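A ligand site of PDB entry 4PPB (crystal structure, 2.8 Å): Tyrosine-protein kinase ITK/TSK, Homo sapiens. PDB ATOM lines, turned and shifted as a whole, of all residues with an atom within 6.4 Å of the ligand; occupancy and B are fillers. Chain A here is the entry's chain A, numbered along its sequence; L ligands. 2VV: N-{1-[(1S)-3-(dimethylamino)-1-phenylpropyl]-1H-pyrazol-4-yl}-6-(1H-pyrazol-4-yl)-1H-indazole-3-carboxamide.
The backbone carbonyl oxygen (O) of Glu 82 lies within hydrogen-bond range of a nitrogen (N29) of the ligand. The backbone NH of Met 84 sits at hydrogen-bond distance from a nitrogen (N31) of the ligand (3.0 Å). A nitrogen (N19) of the ligand is in hydrogen-bond range of the backbone carbonyl oxygen (O) of Met 84 (2.9 Å). The side-chain amino group (NZ) of Lys 37 lies close to a nitrogen (N34) of the ligand, at 3.1 Å.
The side-chain amino group (NZ) of Lys 37 lies within salt-bridge range of the side-chain carboxylate (OD2) of Asp 146, 3.6 Å away. N of Phe 81 is in hydrogen-bond range of O of Ala 35 (2.8 Å). N of His 86 lies within hydrogen-bond range of O of Val 136 (2.9 Å). O of Gly 87 sits at hydrogen-bond distance from N of Val 136, 2.9 Å away.
Residues that only touch the ligand: Ala 35, Val 65, Phe 81, Phe 83, Glu 85, His 86, Gly 87, Leu 135, Ser 145 and Asp 146. Within 4 Å of the ligand: Ala 35, Lys 37, Val 65, Phe 81, Glu 82, Phe 83, Met 84, Glu 85, His 86, Gly 87, Leu 135, Ser 145 and Asp 146.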
ATOM      1  N   LYS A  33      22.038 -16.580 -28.331  1.00  0.00           N
ATOM      2  CA  LYS A  33      21.481 -15.618 -27.370  1.00  0.00           C
ATOM      3  C   LYS A  33      21.803 -16.099 -25.964  1.00  0.00           C
ATOM      4  O   LYS A  33      21.753 -17.297 -25.701  1.00  0.00           O
ATOM      5  CB  LYS A  33      19.943 -15.511 -27.513  1.00  0.00           C
ATOM      6  CG  LYS A  33      19.463 -14.962 -28.843  1.00  0.00           C
ATOM      7  CD  LYS A  33      18.010 -14.556 -28.831  1.00  0.00           C
ATOM      8  CE  LYS A  33      17.528 -14.195 -30.212  1.00  0.00           C
ATOM      9  NZ  LYS A  33      16.304 -13.357 -30.190  1.00  0.00           N
ATOM     10  N   VAL A  34      22.171 -15.167 -25.071  1.00  0.00           N
ATOM     11  CA  VAL A  34      22.472 -15.398 -23.654  1.00  0.00           C
ATOM     12  C   VAL A  34      21.942 -14.219 -22.801  1.00  0.00           C
ATOM     13  O   VAL A  34      21.691 -13.136 -23.328  1.00  0.00           O
ATOM     14  CB  VAL A  34      23.977 -15.671 -23.331  1.00  0.00           C
ATOM     15  CG1 VAL A  34      24.429 -17.023 -23.837  1.00  0.00           C
ATOM     16  CG2 VAL A  34      24.889 -14.559 -23.853  1.00  0.00           C
ATOM     17  N   ALA A  35      21.787 -14.444 -21.492  1.00  0.00           N
ATOM     18  CA  ALA A  35      21.406 -13.422 -20.524  1.00  0.00           C
ATOM     19  C   ALA A  35      22.667 -13.142 -19.713  1.00  0.00           C
ATOM     20  O   ALA A  35      23.338 -14.082 -19.272  1.00  0.00           O
ATOM     21  CB  ALA A  35      20.305 -13.915 -19.625  1.00  0.00           C
ATOM     22  N   LYS A  37      24.222 -11.089 -16.476  1.00  0.00           N
ATOM     23  CA  LYS A  37      23.996 -10.443 -15.188  1.00  0.00           C
ATOM     24  C   LYS A  37      25.211  -9.616 -14.826  1.00  0.00           C
ATOM     25  O   LYS A  37      26.337 -10.102 -14.934  1.00  0.00           O
ATOM     26  CB  LYS A  37      23.693 -11.491 -14.104  1.00  0.00           C
ATOM     27  CG  LYS A  37      23.049 -10.962 -12.834  1.00  0.00           C
ATOM     28  CD  LYS A  37      22.851 -12.108 -11.864  1.00  0.00           C
ATOM     29  CE  LYS A  37      22.102 -11.749 -10.604  1.00  0.00           C
ATOM     30  NZ  LYS A  37      20.666 -11.456 -10.864  1.00  0.00           N
ATOM     31  N   MET A  56      28.551 -23.332  -9.111  1.00  0.00           N
ATOM     32  CA  MET A  56      27.282 -23.128  -9.822  1.00  0.00           C
ATOM     33  C   MET A  56      27.269 -23.833 -11.183  1.00  0.00           C
ATOM     34  O   MET A  56      26.194 -24.178 -11.683  1.00  0.00           O
ATOM     35  CB  MET A  56      27.009 -21.624 -10.003  1.00  0.00           C
ATOM     36  CG  MET A  56      26.177 -21.002  -8.902  1.00  0.00           C
ATOM     37  SD  MET A  56      25.395 -19.434  -9.410  1.00  0.00           S
ATOM     38  CE  MET A  56      23.925 -20.060 -10.289  1.00  0.00           C
ATOM     39  N   VAL A  65      18.076 -22.566 -14.463  1.00  0.00           N
ATOM     40  CA  VAL A  65      18.716 -21.660 -15.414  1.00  0.00           C
ATOM     41  C   VAL A  65      20.222 -21.870 -15.309  1.00  0.00           C
ATOM     42  O   VAL A  65      20.827 -21.644 -14.244  1.00  0.00           O
ATOM     43  CB  VAL A  65      18.279 -20.189 -15.238  1.00  0.00           C
ATOM     44  CG1 VAL A  65      19.187 -19.245 -16.032  1.00  0.00           C
ATOM     45  CG2 VAL A  65      16.834 -20.006 -15.669  1.00  0.00           C
ATOM     46  N   PHE A  81      24.451 -16.463 -18.439  1.00  0.00           N
ATOM     47  CA  PHE A  81      23.401 -17.431 -18.166  1.00  0.00           C
ATOM     48  C   PHE A  81      22.674 -17.851 -19.419  1.00  0.00           C
ATOM     49  O   PHE A  81      22.780 -17.206 -20.455  1.00  0.00           O
ATOM     50  CB  PHE A  81      22.384 -16.856 -17.165  1.00  0.00           C
ATOM     51  CG  PHE A  81      22.882 -16.844 -15.740  1.00  0.00           C
ATOM     52  CD1 PHE A  81      23.264 -15.648 -15.129  1.00  0.00           C
ATOM     53  CD2 PHE A  81      22.963 -18.014 -15.006  1.00  0.00           C
ATOM     54  CE1 PHE A  81      23.725 -15.641 -13.813  1.00  0.00           C
ATOM     55  CE2 PHE A  81      23.424 -18.008 -13.690  1.00  0.00           C
ATOM     56  CZ  PHE A  81      23.817 -16.825 -13.107  1.00  0.00           C
ATOM     57  N   GLU A  82      21.906 -18.927 -19.291  1.00  0.00           N
ATOM     58  CA  GLU A  82      21.035 -19.495 -20.314  1.00  0.00           C
ATOM     59  C   GLU A  82      19.922 -18.472 -20.630  1.00  0.00           C
ATOM     60  O   GLU A  82      19.289 -17.958 -19.702  1.00  0.00           O
ATOM     61  CB  GLU A  82      20.432 -20.777 -19.751  1.00  0.00           C
ATOM     62  CG  GLU A  82      19.516 -21.516 -20.702  1.00  0.00           C
ATOM     63  CD  GLU A  82      18.704 -22.614 -20.050  1.00  0.00           C
ATOM     64  OE1 GLU A  82      17.649 -22.964 -20.618  1.00  0.00           O
ATOM     65  OE2 GLU A  82      19.127 -23.130 -18.982  1.00  0.00           O
ATOM     66  N   PHE A  83      19.688 -18.175 -21.919  1.00  0.00           N
ATOM     67  CA  PHE A  83      18.607 -17.250 -22.283  1.00  0.00           C
ATOM     68  C   PHE A  83      17.251 -17.948 -22.190  1.00  0.00           C
ATOM     69  O   PHE A  83      17.089 -19.080 -22.678  1.00  0.00           O
ATOM     70  CB  PHE A  83      18.828 -16.619 -23.673  1.00  0.00           C
ATOM     71  CG  PHE A  83      17.774 -15.604 -24.040  1.00  0.00           C
ATOM     72  CD1 PHE A  83      17.709 -14.369 -23.394  1.00  0.00           C
ATOM     73  CD2 PHE A  83      16.830 -15.879 -25.022  1.00  0.00           C
ATOM     74  CE1 PHE A  83      16.719 -13.445 -23.724  1.00  0.00           C
ATOM     75  CE2 PHE A  83      15.845 -14.948 -25.356  1.00  0.00           C
ATOM     76  CZ  PHE A  83      15.799 -13.736 -24.703  1.00  0.00           C
ATOM     77  N   MET A  84      16.276 -17.291 -21.524  1.00  0.00           N
ATOM     78  CA  MET A  84      14.925 -17.812 -21.310  1.00  0.00           C
ATOM     79  C   MET A  84      13.921 -16.967 -22.083  1.00  0.00           C
ATOM     80  O   MET A  84      13.479 -15.934 -21.599  1.00  0.00           O
ATOM     81  CB  MET A  84      14.612 -17.905 -19.810  1.00  0.00           C
ATOM     82  CG  MET A  84      15.494 -18.884 -19.054  1.00  0.00           C
ATOM     83  SD  MET A  84      15.360 -20.595 -19.616  1.00  0.00           S
ATOM     84  CE  MET A  84      13.756 -21.042 -18.963  1.00  0.00           C
ATOM     85  N   GLU A  85      13.583 -17.436 -23.279  1.00  0.00           N
ATOM     86  CA  GLU A  85      12.730 -16.846 -24.326  1.00  0.00           C
ATOM     87  C   GLU A  85      11.536 -15.994 -23.857  1.00  0.00           C
ATOM     88  O   GLU A  85      11.305 -14.956 -24.472  1.00  0.00           O
ATOM     89  CB  GLU A  85      12.234 -17.965 -25.279  1.00  0.00           C
ATOM     90  CG  GLU A  85      11.744 -17.526 -26.656  1.00  0.00           C
ATOM     91  CD  GLU A  85      12.693 -16.763 -27.547  1.00  0.00           C
ATOM     92  OE1 GLU A  85      13.860 -17.193 -27.694  1.00  0.00           O
ATOM     93  OE2 GLU A  85      12.269 -15.743 -28.146  1.00  0.00           O
ATOM     94  N   HIS A  86      10.800 -16.382 -22.809  1.00  0.00           N
ATOM     95  CA  HIS A  86       9.582 -15.651 -22.420  1.00  0.00           C
ATOM     96  C   HIS A  86       9.684 -14.762 -21.148  1.00  0.00           C
ATOM     97  O   HIS A  86       8.678 -14.149 -20.768  1.00  0.00           O
ATOM     98  CB  HIS A  86       8.400 -16.623 -22.314  1.00  0.00           C
ATOM     99  CG  HIS A  86       8.131 -17.345 -23.603  1.00  0.00           C
ATOM    100  ND1 HIS A  86       7.694 -16.668 -24.739  1.00  0.00           N
ATOM    101  CD2 HIS A  86       8.320 -18.643 -23.916  1.00  0.00           C
ATOM    102  CE1 HIS A  86       7.598 -17.584 -25.691  1.00  0.00           C
ATOM    103  NE2 HIS A  86       7.974 -18.798 -25.243  1.00  0.00           N
ATOM    104  N   GLY A  87      10.861 -14.634 -20.548  1.00  0.00           N
ATOM    105  CA  GLY A  87      11.052 -13.787 -19.367  1.00  0.00           C
ATOM    106  C   GLY A  87      10.560 -14.362 -18.060  1.00  0.00           C
ATOM    107  O   GLY A  87      10.429 -15.583 -17.920  1.00  0.00           O
ATOM    108  N   CYS A  88      10.306 -13.478 -17.054  1.00  0.00           N
ATOM    109  CA  CYS A  88       9.885 -13.930 -15.720  1.00  0.00           C
ATOM    110  C   CYS A  88       8.436 -14.442 -15.681  1.00  0.00           C
ATOM    111  O   CYS A  88       7.564 -13.909 -16.355  1.00  0.00           O
ATOM    112  CB  CYS A  88      10.158 -12.898 -14.636  1.00  0.00           C
ATOM    113  SG  CYS A  88       9.188 -11.370 -14.762  1.00  0.00           S
ATOM    114  N   TYR A  92       4.594 -13.215 -16.906  1.00  0.00           N
ATOM    115  CA  TYR A  92       4.039 -14.167 -17.863  1.00  0.00           C
ATOM    116  C   TYR A  92       2.626 -14.590 -17.448  1.00  0.00           C
ATOM    117  O   TYR A  92       1.711 -14.626 -18.297  1.00  0.00           O
ATOM    118  CB  TYR A  92       4.971 -15.370 -18.028  1.00  0.00           C
ATOM    119  CG  TYR A  92       4.503 -16.335 -19.098  1.00  0.00           C
ATOM    120  CD1 TYR A  92       4.876 -16.156 -20.429  1.00  0.00           C
ATOM    121  CD2 TYR A  92       3.676 -17.411 -18.785  1.00  0.00           C
ATOM    122  CE1 TYR A  92       4.422 -17.027 -21.428  1.00  0.00           C
ATOM    123  CE2 TYR A  92       3.213 -18.282 -19.773  1.00  0.00           C
ATOM    124  CZ  TYR A  92       3.602 -18.091 -21.090  1.00  0.00           C
ATOM    125  OH  TYR A  92       3.156 -18.957 -22.053  1.00  0.00           O
ATOM    126  N   THR A  95       0.010 -11.428 -17.749  1.00  0.00           N
ATOM    127  CA  THR A  95      -0.430 -11.064 -19.101  1.00  0.00           C
ATOM    128  C   THR A  95      -1.416 -12.091 -19.696  1.00  0.00           C
ATOM    129  O   THR A  95      -2.267 -11.707 -20.503  1.00  0.00           O
ATOM    130  CB  THR A  95       0.746 -10.772 -20.047  1.00  0.00           C
ATOM    131  OG1 THR A  95       1.505 -11.947 -20.272  1.00  0.00           O
ATOM    132  CG2 THR A  95       1.657  -9.666 -19.538  1.00  0.00           C
ATOM    133  N   LEU A 135      11.759 -18.491 -14.554  1.00  0.00           N
ATOM    134  CA  LEU A 135      11.704 -18.015 -15.928  1.00  0.00           C
ATOM    135  C   LEU A 135      11.061 -18.983 -16.880  1.00  0.00           C
ATOM    136  O   LEU A 135      11.207 -20.194 -16.716  1.00  0.00           O
ATOM    137  CB  LEU A 135      13.111 -17.623 -16.415  1.00  0.00           C
ATOM    138  CG  LEU A 135      13.772 -16.443 -15.695  1.00  0.00           C
ATOM    139  CD1 LEU A 135      15.230 -16.667 -15.538  1.00  0.00           C
ATOM    140  CD2 LEU A 135      13.548 -15.143 -16.434  1.00  0.00           C
ATOM    141  N   VAL A 136      10.356 -18.448 -17.888  1.00  0.00           N
ATOM    142  CA  VAL A 136       9.661 -19.223 -18.923  1.00  0.00           C
ATOM    143  C   VAL A 136      10.534 -19.334 -20.185  1.00  0.00           C
ATOM    144  O   VAL A 136      11.002 -18.310 -20.690  1.00  0.00           O
ATOM    145  CB  VAL A 136       8.244 -18.666 -19.232  1.00  0.00           C
ATOM    146  CG1 VAL A 136       7.399 -19.714 -19.956  1.00  0.00           C
ATOM    147  CG2 VAL A 136       7.536 -18.181 -17.971  1.00  0.00           C
ATOM    148  N   SER A 145      15.796 -19.796 -11.178  1.00  0.00           N
ATOM    149  CA  SER A 145      16.958 -18.916 -11.273  1.00  0.00           C
ATOM    150  C   SER A 145      17.213 -18.150  -9.978  1.00  0.00           C
ATOM    151  O   SER A 145      16.391 -18.213  -9.064  1.00  0.00           O
ATOM    152  CB  SER A 145      16.838 -17.964 -12.455  1.00  0.00           C
ATOM    153  OG  SER A 145      16.167 -16.759 -12.131  1.00  0.00           O
ATOM    154  N   ASP A 146      18.346 -17.421  -9.911  1.00  0.00           N
ATOM    155  CA  ASP A 146      18.817 -16.586  -8.801  1.00  0.00           C
ATOM    156  C   ASP A 146      19.087 -17.390  -7.511  1.00  0.00           C
ATOM    157  O   ASP A 146      18.674 -16.998  -6.423  1.00  0.00           O
ATOM    158  CB  ASP A 146      17.887 -15.382  -8.549  1.00  0.00           C
ATOM    159  CG  ASP A 146      18.563 -14.037  -8.691  1.00  0.00           C
ATOM    160  OD1 ASP A 146      19.731 -13.893  -8.242  1.00  0.00           O
ATOM    161  OD2 ASP A 146      17.907 -13.100  -9.223  1.00  0.00           O
ATOM    162  N   PHE A 147      19.833 -18.497  -7.652  1.00  0.00           N
ATOM    163  CA  PHE A 147      20.201 -19.340  -6.521  1.00  0.00           C
ATOM    164  C   PHE A 147      21.711 -19.238  -6.306  1.00  0.00           C
ATOM    165  O   PHE A 147      22.496 -19.586  -7.201  1.00  0.00           O
ATOM    166  CB  PHE A 147      19.695 -20.790  -6.684  1.00  0.00           C
ATOM    167  CG  PHE A 147      19.970 -21.457  -8.013  1.00  0.00           C
ATOM    168  CD1 PHE A 147      21.033 -22.335  -8.162  1.00  0.00           C
ATOM    169  CD2 PHE A 147      19.143 -21.243  -9.106  1.00  0.00           C
ATOM    170  CE1 PHE A 147      21.280 -22.979  -9.383  1.00  0.00           C
ATOM    171  CE2 PHE A 147      19.396 -21.865 -10.331  1.00  0.00           C
ATOM    172  CZ  PHE A 147      20.458 -22.730 -10.461  1.00  0.00           C
HETATM  173  C1  2VV L   1       7.544  -9.478 -22.618  1.00  0.00           C
HETATM  174  N2  2VV L   1       8.243 -10.768 -22.746  1.00  0.00           N
HETATM  175  C3  2VV L   1       7.305 -11.890 -22.868  1.00  0.00           C
HETATM  176  C4  2VV L   1       9.215 -10.788 -23.850  1.00  0.00           C
HETATM  177  C5  2VV L   1      10.613 -10.515 -23.296  1.00  0.00           C
HETATM  178  C6  2VV L   1      11.653 -11.575 -23.696  1.00  0.00           C
HETATM  179  C8  2VV L   1      12.619 -11.051 -24.755  1.00  0.00           C
HETATM  180  C9  2VV L   1      12.913 -11.839 -25.867  1.00  0.00           C
HETATM  181  C10 2VV L   1      13.832 -11.396 -26.826  1.00  0.00           C
HETATM  182  C11 2VV L   1      14.469 -10.173 -26.671  1.00  0.00           C
HETATM  183  C12 2VV L   1      14.194  -9.380 -25.550  1.00  0.00           C
HETATM  184  C13 2VV L   1      13.292  -9.824 -24.596  1.00  0.00           C
HETATM  185  N14 2VV L   1      12.491 -11.852 -22.518  1.00  0.00           N
HETATM  186  C15 2VV L   1      13.320 -12.907 -22.326  1.00  0.00           C
HETATM  187  C16 2VV L   1      13.935 -12.725 -21.128  1.00  0.00           C
HETATM  188  C17 2VV L   1      13.524 -11.489 -20.624  1.00  0.00           C
HETATM  189  N18 2VV L   1      12.670 -10.962 -21.453  1.00  0.00           N
HETATM  190  N19 2VV L   1      14.856 -13.613 -20.508  1.00  0.00           N
HETATM  191  C20 2VV L   1      15.426 -13.357 -19.312  1.00  0.00           C
HETATM  192  O21 2VV L   1      15.179 -12.322 -18.699  1.00  0.00           O
HETATM  193  C22 2VV L   1      16.428 -14.296 -18.743  1.00  0.00           C
HETATM  194  C23 2VV L   1      17.074 -14.166 -17.421  1.00  0.00           C
HETATM  195  C24 2VV L   1      16.959 -13.280 -16.346  1.00  0.00           C
HETATM  196  C25 2VV L   1      17.738 -13.450 -15.239  1.00  0.00           C
HETATM  197  C26 2VV L   1      18.669 -14.511 -15.175  1.00  0.00           C
HETATM  198  C27 2VV L   1      18.758 -15.432 -16.226  1.00  0.00           C
HETATM  199  C28 2VV L   1      17.975 -15.259 -17.374  1.00  0.00           C
HETATM  200  N29 2VV L   1      17.831 -15.924 -18.569  1.00  0.00           N
HETATM  201  N31 2VV L   1      16.954 -15.357 -19.323  1.00  0.00           N
HETATM  202  C32 2VV L   1      19.440 -14.711 -13.914  1.00  0.00           C
HETATM  203  C33 2VV L   1      19.765 -13.764 -13.002  1.00  0.00           C
HETATM  204  N34 2VV L   1      20.419 -14.375 -11.993  1.00  0.00           N
HETATM  205  N36 2VV L   1      20.510 -15.740 -12.281  1.00  0.00           N
HETATM  206  C37 2VV L   1      19.917 -15.947 -13.431  1.00  0.00           C
